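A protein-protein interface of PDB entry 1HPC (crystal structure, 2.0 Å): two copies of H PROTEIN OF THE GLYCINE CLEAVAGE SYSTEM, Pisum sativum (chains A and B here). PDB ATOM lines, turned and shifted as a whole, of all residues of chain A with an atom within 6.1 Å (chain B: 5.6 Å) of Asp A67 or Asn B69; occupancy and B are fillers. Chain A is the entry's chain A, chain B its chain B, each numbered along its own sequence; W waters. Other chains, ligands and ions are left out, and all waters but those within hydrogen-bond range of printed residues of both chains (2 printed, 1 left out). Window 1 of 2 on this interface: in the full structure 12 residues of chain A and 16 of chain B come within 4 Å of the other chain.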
ATOM      1  N   GLU A  14      20.812  30.143   4.742  1.00  0.00           N
ATOM      2  CA  GLU A  14      19.623  29.522   5.319  1.00  0.00           C
ATOM      3  C   GLU A  14      19.755  29.759   6.814  1.00  0.00           C
ATOM      4  O   GLU A  14      20.882  29.876   7.328  1.00  0.00           O
ATOM      5  CB  GLU A  14      19.533  27.987   5.151  1.00  0.00           C
ATOM      6  CG  GLU A  14      19.347  27.376   3.754  1.00  0.00           C
ATOM      7  CD  GLU A  14      20.594  27.352   2.884  1.00  0.00           C
ATOM      8  OE1 GLU A  14      21.690  27.117   3.403  1.00  0.00           O
ATOM      9  OE2 GLU A  14      20.466  27.560   1.680  1.00  0.00           O
ATOM     10  N   GLU A  42       9.814  25.047  -4.389  1.00  0.00           N
ATOM     11  CA  GLU A  42       9.633  23.603  -4.462  1.00  0.00           C
ATOM     12  C   GLU A  42      10.069  23.004  -3.119  1.00  0.00           C
ATOM     13  O   GLU A  42      11.207  23.229  -2.684  1.00  0.00           O
ATOM     14  CB  GLU A  42      10.482  23.044  -5.589  1.00  0.00           C
ATOM     15  CG  GLU A  42      10.009  23.586  -6.916  1.00  0.00           C
ATOM     16  CD  GLU A  42      10.858  23.061  -8.055  1.00  0.00           C
ATOM     17  OE1 GLU A  42      11.874  23.685  -8.370  1.00  0.00           O
ATOM     18  OE2 GLU A  42      10.503  22.029  -8.617  1.00  0.00           O
ATOM     19  N   GLY A  55      20.782  19.419  -0.903  1.00  0.00           N
ATOM     20  CA  GLY A  55      19.615  20.204  -1.264  1.00  0.00           C
ATOM     21  C   GLY A  55      18.333  19.496  -0.894  1.00  0.00           C
ATOM     22  O   GLY A  55      18.227  18.270  -1.018  1.00  0.00           O
ATOM     23  N   GLY A  57      15.202  21.475  -1.632  1.00  0.00           N
ATOM     24  CA  GLY A  57      14.157  22.150  -2.362  1.00  0.00           C
ATOM     25  C   GLY A  57      14.746  23.260  -3.189  1.00  0.00           C
ATOM     26  O   GLY A  57      15.976  23.333  -3.310  1.00  0.00           O
ATOM     27  N   ALA A  58      13.947  24.178  -3.698  1.00  0.00           N
ATOM     28  CA  ALA A  58      14.452  25.228  -4.562  1.00  0.00           C
ATOM     29  C   ALA A  58      13.553  26.437  -4.466  1.00  0.00           C
ATOM     30  O   ALA A  58      12.355  26.312  -4.213  1.00  0.00           O
ATOM     31  CB  ALA A  58      14.458  24.811  -6.027  1.00  0.00           C
ATOM     32  N   VAL A  59      14.152  27.611  -4.669  1.00  0.00           N
ATOM     33  CA  VAL A  59      13.436  28.873  -4.679  1.00  0.00           C
ATOM     34  C   VAL A  59      13.670  29.426  -6.082  1.00  0.00           C
ATOM     35  O   VAL A  59      14.792  29.397  -6.577  1.00  0.00           O
ATOM     36  CB  VAL A  59      14.038  29.794  -3.577  1.00  0.00           C
ATOM     37  CG1 VAL A  59      13.345  31.123  -3.565  1.00  0.00           C
ATOM     38  CG2 VAL A  59      13.796  29.192  -2.204  1.00  0.00           C
ATOM     39  N   GLU A  60      12.643  29.893  -6.771  1.00  0.00           N
ATOM     40  CA  GLU A  60      12.796  30.445  -8.102  1.00  0.00           C
ATOM     41  C   GLU A  60      12.390  31.894  -8.073  1.00  0.00           C
ATOM     42  O   GLU A  60      11.308  32.251  -7.581  1.00  0.00           O
ATOM     43  CB  GLU A  60      11.908  29.776  -9.146  1.00  0.00           C
ATOM     44  CG  GLU A  60      12.450  28.461  -9.692  1.00  0.00           C
ATOM     45  CD  GLU A  60      11.915  27.210  -9.006  1.00  0.00           C
ATOM     46  OE1 GLU A  60      10.701  26.996  -9.000  1.00  0.00           O
ATOM     47  OE2 GLU A  60      12.720  26.435  -8.496  1.00  0.00           O
ATOM     48  N   THR A  65      16.979  30.009 -10.681  1.00  0.00           N
ATOM     49  CA  THR A  65      16.653  28.933  -9.741  1.00  0.00           C
ATOM     50  C   THR A  65      17.793  28.869  -8.728  1.00  0.00           C
ATOM     51  O   THR A  65      18.975  28.850  -9.088  1.00  0.00           O
ATOM     52  CB  THR A  65      16.570  27.527 -10.423  1.00  0.00           C
ATOM     53  OG1 THR A  65      15.534  27.605 -11.390  1.00  0.00           O
ATOM     54  CG2 THR A  65      16.294  26.391  -9.447  1.00  0.00           C
ATOM     55  N   SER A  66      17.463  28.783  -7.455  1.00  0.00           N
ATOM     56  CA  SER A  66      18.449  28.641  -6.412  1.00  0.00           C
ATOM     57  C   SER A  66      18.098  27.408  -5.570  1.00  0.00           C
ATOM     58  O   SER A  66      17.056  27.385  -4.909  1.00  0.00           O
ATOM     59  CB  SER A  66      18.406  29.944  -5.621  1.00  0.00           C
ATOM     60  OG  SER A  66      19.368  30.032  -4.589  1.00  0.00           O
ATOM     61  N   ASP A  67      18.926  26.367  -5.534  1.00  0.00           N
ATOM     62  CA  ASP A  67      18.620  25.173  -4.760  1.00  0.00           C
ATOM     63  C   ASP A  67      19.039  25.454  -3.346  1.00  0.00           C
ATOM     64  O   ASP A  67      20.049  26.132  -3.130  1.00  0.00           O
ATOM     65  CB  ASP A  67      19.371  23.967  -5.293  1.00  0.00           C
ATOM     66  CG  ASP A  67      18.872  23.546  -6.659  1.00  0.00           C
ATOM     67  OD1 ASP A  67      17.701  23.739  -6.976  1.00  0.00           O
ATOM     68  OD2 ASP A  67      19.662  23.025  -7.416  1.00  0.00           O
ATOM     69  N   VAL A  68      18.207  25.023  -2.398  1.00  0.00           N
ATOM     70  CA  VAL A  68      18.453  25.332  -0.993  1.00  0.00           C
ATOM     71  C   VAL A  68      18.926  24.083  -0.293  1.00  0.00           C
ATOM     72  O   VAL A  68      18.330  23.013  -0.429  1.00  0.00           O
ATOM     73  CB  VAL A  68      17.163  25.905  -0.302  1.00  0.00           C
ATOM     74  CG1 VAL A  68      16.817  27.238  -0.903  1.00  0.00           C
ATOM     75  CG2 VAL A  68      15.951  25.077  -0.570  1.00  0.00           C
ATOM     76  N   ASN A  69      20.027  24.222   0.422  1.00  0.00           N
ATOM     77  CA  ASN A  69      20.653  23.095   1.118  1.00  0.00           C
ATOM     78  C   ASN A  69      20.171  23.005   2.543  1.00  0.00           C
ATOM     79  O   ASN A  69      19.945  24.054   3.154  1.00  0.00           O
ATOM     80  CB  ASN A  69      22.156  23.218   1.194  1.00  0.00           C
ATOM     81  CG  ASN A  69      22.817  23.124  -0.162  1.00  0.00           C
ATOM     82  OD1 ASN A  69      22.318  22.483  -1.085  1.00  0.00           O
ATOM     83  ND2 ASN A  69      23.938  23.836  -0.286  1.00  0.00           N
ATOM     84  N   SER B  12      11.041  24.541 -12.730  1.00  0.00           N
ATOM     85  CA  SER B  12      12.299  25.266 -12.709  1.00  0.00           C
ATOM     86  C   SER B  12      12.838  25.569 -14.096  1.00  0.00           C
ATOM     87  O   SER B  12      13.971  26.022 -14.272  1.00  0.00           O
ATOM     88  CB  SER B  12      13.304  24.470 -11.895  1.00  0.00           C
ATOM     89  OG  SER B  12      13.200  23.101 -12.192  1.00  0.00           O
ATOM     90  N   GLU B  14      13.307  23.680 -17.099  1.00  0.00           N
ATOM     91  CA  GLU B  14      14.059  22.757 -17.931  1.00  0.00           C
ATOM     92  C   GLU B  14      13.037  21.956 -18.732  1.00  0.00           C
ATOM     93  O   GLU B  14      11.898  21.799 -18.277  1.00  0.00           O
ATOM     94  CB  GLU B  14      14.887  21.750 -17.139  1.00  0.00           C
ATOM     95  CG  GLU B  14      15.925  22.336 -16.178  1.00  0.00           C
ATOM     96  CD  GLU B  14      15.392  22.695 -14.796  1.00  0.00           C
ATOM     97  OE1 GLU B  14      14.300  22.273 -14.430  1.00  0.00           O
ATOM     98  OE2 GLU B  14      16.097  23.383 -14.067  1.00  0.00           O
ATOM     99  N   ILE B  25      17.919  16.837 -22.105  1.00  0.00           N
ATOM    100  CA  ILE B  25      17.487  17.894 -21.200  1.00  0.00           C
ATOM    101  C   ILE B  25      18.169  19.229 -21.531  1.00  0.00           C
ATOM    102  O   ILE B  25      19.346  19.264 -21.890  1.00  0.00           O
ATOM    103  CB  ILE B  25      17.815  17.429 -19.739  1.00  0.00           C
ATOM    104  CG1 ILE B  25      16.951  16.235 -19.379  1.00  0.00           C
ATOM    105  CG2 ILE B  25      17.533  18.557 -18.732  1.00  0.00           C
ATOM    106  CD1 ILE B  25      17.543  15.368 -18.256  1.00  0.00           C
ATOM    107  N   GLY B  53      14.548  16.774  -9.398  1.00  0.00           N
ATOM    108  CA  GLY B  53      14.561  17.886  -8.468  1.00  0.00           C
ATOM    109  C   GLY B  53      15.942  18.269  -7.958  1.00  0.00           C
ATOM    110  O   GLY B  53      16.056  19.309  -7.318  1.00  0.00           O
ATOM    111  N   LYS B  54      17.008  17.516  -8.204  1.00  0.00           N
ATOM    112  CA  LYS B  54      18.323  17.869  -7.708  1.00  0.00           C
ATOM    113  C   LYS B  54      19.119  18.514  -8.833  1.00  0.00           C
ATOM    114  O   LYS B  54      19.017  18.084  -9.994  1.00  0.00           O
ATOM    115  CB  LYS B  54      19.087  16.648  -7.249  1.00  0.00           C
ATOM    116  CG  LYS B  54      18.374  15.811  -6.217  1.00  0.00           C
ATOM    117  CD  LYS B  54      18.474  16.448  -4.846  1.00  0.00           C
ATOM    118  CE  LYS B  54      17.794  15.556  -3.818  1.00  0.00           C
ATOM    119  NZ  LYS B  54      16.347  15.623  -3.952  1.00  0.00           N
ATOM    120  N   GLY B  55      19.930  19.524  -8.492  1.00  0.00           N
ATOM    121  CA  GLY B  55      20.787  20.226  -9.440  1.00  0.00           C
ATOM    122  C   GLY B  55      21.868  19.334 -10.027  1.00  0.00           C
ATOM    123  O   GLY B  55      22.454  18.508  -9.323  1.00  0.00           O
ATOM    124  N   PHE B  56      22.091  19.429 -11.333  1.00  0.00           N
ATOM    125  CA  PHE B  56      23.172  18.695 -11.952  1.00  0.00           C
ATOM    126  C   PHE B  56      24.196  19.638 -12.535  1.00  0.00           C
ATOM    127  O   PHE B  56      25.247  19.206 -12.975  1.00  0.00           O
ATOM    128  CB  PHE B  56      22.660  17.781 -13.068  1.00  0.00           C
ATOM    129  CG  PHE B  56      21.975  18.422 -14.272  1.00  0.00           C
ATOM    130  CD1 PHE B  56      22.726  18.999 -15.318  1.00  0.00           C
ATOM    131  CD2 PHE B  56      20.588  18.406 -14.335  1.00  0.00           C
ATOM    132  CE1 PHE B  56      22.087  19.558 -16.418  1.00  0.00           C
ATOM    133  CE2 PHE B  56      19.954  18.966 -15.447  1.00  0.00           C
ATOM    134  CZ  PHE B  56      20.697  19.538 -16.481  1.00  0.00           C
ATOM    135  N   GLY B  57      23.918  20.936 -12.593  1.00  0.00           N
ATOM    136  CA  GLY B  57      24.835  21.834 -13.232  1.00  0.00           C
ATOM    137  C   GLY B  57      24.383  23.221 -12.939  1.00  0.00           C
ATOM    138  O   GLY B  57      23.504  23.422 -12.102  1.00  0.00           O
ATOM    139  N   ASP B  67      20.941  27.485 -10.840  1.00  0.00           N
ATOM    140  CA  ASP B  67      21.096  26.042 -10.749  1.00  0.00           C
ATOM    141  C   ASP B  67      20.192  25.376 -11.773  1.00  0.00           C
ATOM    142  O   ASP B  67      19.093  25.870 -12.035  1.00  0.00           O
ATOM    143  CB  ASP B  67      20.711  25.519  -9.389  1.00  0.00           C
ATOM    144  CG  ASP B  67      21.694  25.938  -8.321  1.00  0.00           C
ATOM    145  OD1 ASP B  67      22.889  25.810  -8.530  1.00  0.00           O
ATOM    146  OD2 ASP B  67      21.274  26.394  -7.274  1.00  0.00           O
ATOM    147  N   VAL B  68      20.689  24.318 -12.421  1.00  0.00           N
ATOM    148  CA  VAL B  68      19.903  23.562 -13.372  1.00  0.00           C
ATOM    149  C   VAL B  68      19.622  22.216 -12.714  1.00  0.00           C
ATOM    150  O   VAL B  68      20.555  21.487 -12.380  1.00  0.00           O
ATOM    151  CB  VAL B  68      20.693  23.378 -14.665  1.00  0.00           C
ATOM    152  CG1 VAL B  68      19.833  22.599 -15.655  1.00  0.00           C
ATOM    153  CG2 VAL B  68      21.040  24.736 -15.268  1.00  0.00           C
ATOM    154  N   ASN B  69      18.334  21.912 -12.563  1.00  0.00           N
ATOM    155  CA  ASN B  69      17.800  20.728 -11.897  1.00  0.00           C
ATOM    156  C   ASN B  69      17.308  19.682 -12.868  1.00  0.00           C
ATOM    157  O   ASN B  69      16.689  20.024 -13.885  1.00  0.00           O
ATOM    158  CB  ASN B  69      16.631  21.100 -10.999  1.00  0.00           C
ATOM    159  CG  ASN B  69      17.049  22.029  -9.885  1.00  0.00           C
ATOM    160  OD1 ASN B  69      18.211  22.068  -9.503  1.00  0.00           O
ATOM    161  ND2 ASN B  69      16.142  22.831  -9.351  1.00  0.00           N
ATOM    162  N   SER B  70      17.548  18.405 -12.609  1.00  0.00           N
ATOM    163  CA  SER B  70      17.110  17.369 -13.534  1.00  0.00           C
ATOM    164  C   SER B  70      15.596  17.226 -13.381  1.00  0.00           C
ATOM    165  O   SER B  70      15.124  17.143 -12.233  1.00  0.00           O
ATOM    166  CB  SER B  70      17.784  16.051 -13.206  1.00  0.00           C
ATOM    167  OG  SER B  70      17.713  15.192 -14.344  1.00  0.00           O
ATOM    168  N   PRO B  71      14.778  17.222 -14.446  1.00  0.00           N
ATOM    169  CA  PRO B  71      13.342  16.951 -14.366  1.00  0.00           C
ATOM    170  C   PRO B  71      13.045  15.514 -13.975  1.00  0.00           C
ATOM    171  O   PRO B  71      11.997  15.247 -13.408  1.00  0.00           O
ATOM    172  CB  PRO B  71      12.795  17.275 -15.727  1.00  0.00           C
ATOM    173  CG  PRO B  71      13.894  18.056 -16.422  1.00  0.00           C
ATOM    174  CD  PRO B  71      15.182  17.470 -15.829  1.00  0.00           C
HETATM  175  O   HOH W   1      13.486  21.668  -9.785  1.00  0.00           O
HETATM  176  O   HOH W   2      17.338  20.774  -4.593  1.00  0.00           O
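N of Asp B67 sits at hydrogen-bond distance from O of Thr A65.
The backbone NH of Asp A67 lies within hydrogen-bond range of the side-chain carboxylate of Asp B67 (2.9 Å).
The side-chain amide oxygen of Asn B69 sits close to the side-chain carboxylate of Asp A67, 2.7 Å away.
N of Glu A42 lies within hydrogen-bond range of O of Ala A58 (2.8 Å).
N of Gly A55 lies within hydrogen-bond range of OD1 of Asn A69, at 3.4 Å.
The backbone carbonyl oxygen of Val A59 lies within hydrogen-bond range of the backbone NH of Ser A66 (2.9 Å).
OG of Ser B12 lies within hydrogen-bond range of OE1 of Glu B14, at 2.6 Å.
OE2 of Glu B14 lies within hydrogen-bond range of N of Asn B69.
N of Ser B70 lies within hydrogen-bond range of O of Lys B54, at 3.0 Å.
Among the printed residues, merely in contact across the chains: Thr A65 with Asn B69, Asp A67 with Gly B55, Thr A65 with Ser B12, Ser A66 with Asp B67, Glu A42 with Ser B12, Gly A55 with Lys B54 and Glu A60 with Ser B12.
Asp A67 touches just these residues of chain B: Gly B55 (3.6 Å), Asp B67 (2.9 Å) and Asn B69 (2.7 Å).
Of chain A, only Thr A65 and Asp A67 come within 4 Å of Asn B69.
Of the printed residues of chain A, Asp B67 touches Thr A65 (3.0 Å), Ser A66 (3.7 Å) and Asp A67 (2.9 Å).
Of the printed residues of chain B, Gly A55 touches Lys B54 (3.9 Å).
Of the printed residues of chain B, Ser A66 touches Asp B67 (3.7 Å).
Val B68 touches none of the printed residues of chain A.
Ile B25 touches none of the printed residues of chain A.
Of the 13 printed residues of chain B, 5 touch a printed residue of chain A.
Among the printed residues, 10 pairs touch across the chains.
Among the printed residues, no Asp or Glu carboxylate lies within 4 Å of a Lys or Arg side-chain nitrogen of the other chain.
Asp A67 touches Gly B55, but with the chains exchanged Gly A55 does not touch Asp B67 (8.8 Å).
Asp A67 touches its own counterpart, Asp B67.
Asp A67 touches Asn B69, but with the chains exchanged Asn A69 does not touch Asp B67 (7.4 Å).
Positions printed for both chains: 14, 55, 57, 67, 68 and 69.
Water W1 lies within hydrogen-bond range of OG of Ser B12 (2.8 Å), ND2 of Asn B69 (2.9 Å) and OE1 of Glu A42 (2.9 Å).
Water W2 lies within hydrogen-bond range of the backbone carbonyl oxygen of Gly A57 (3.2 Å) and the backbone carbonyl oxygen of Gly B53 (3.3 Å).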
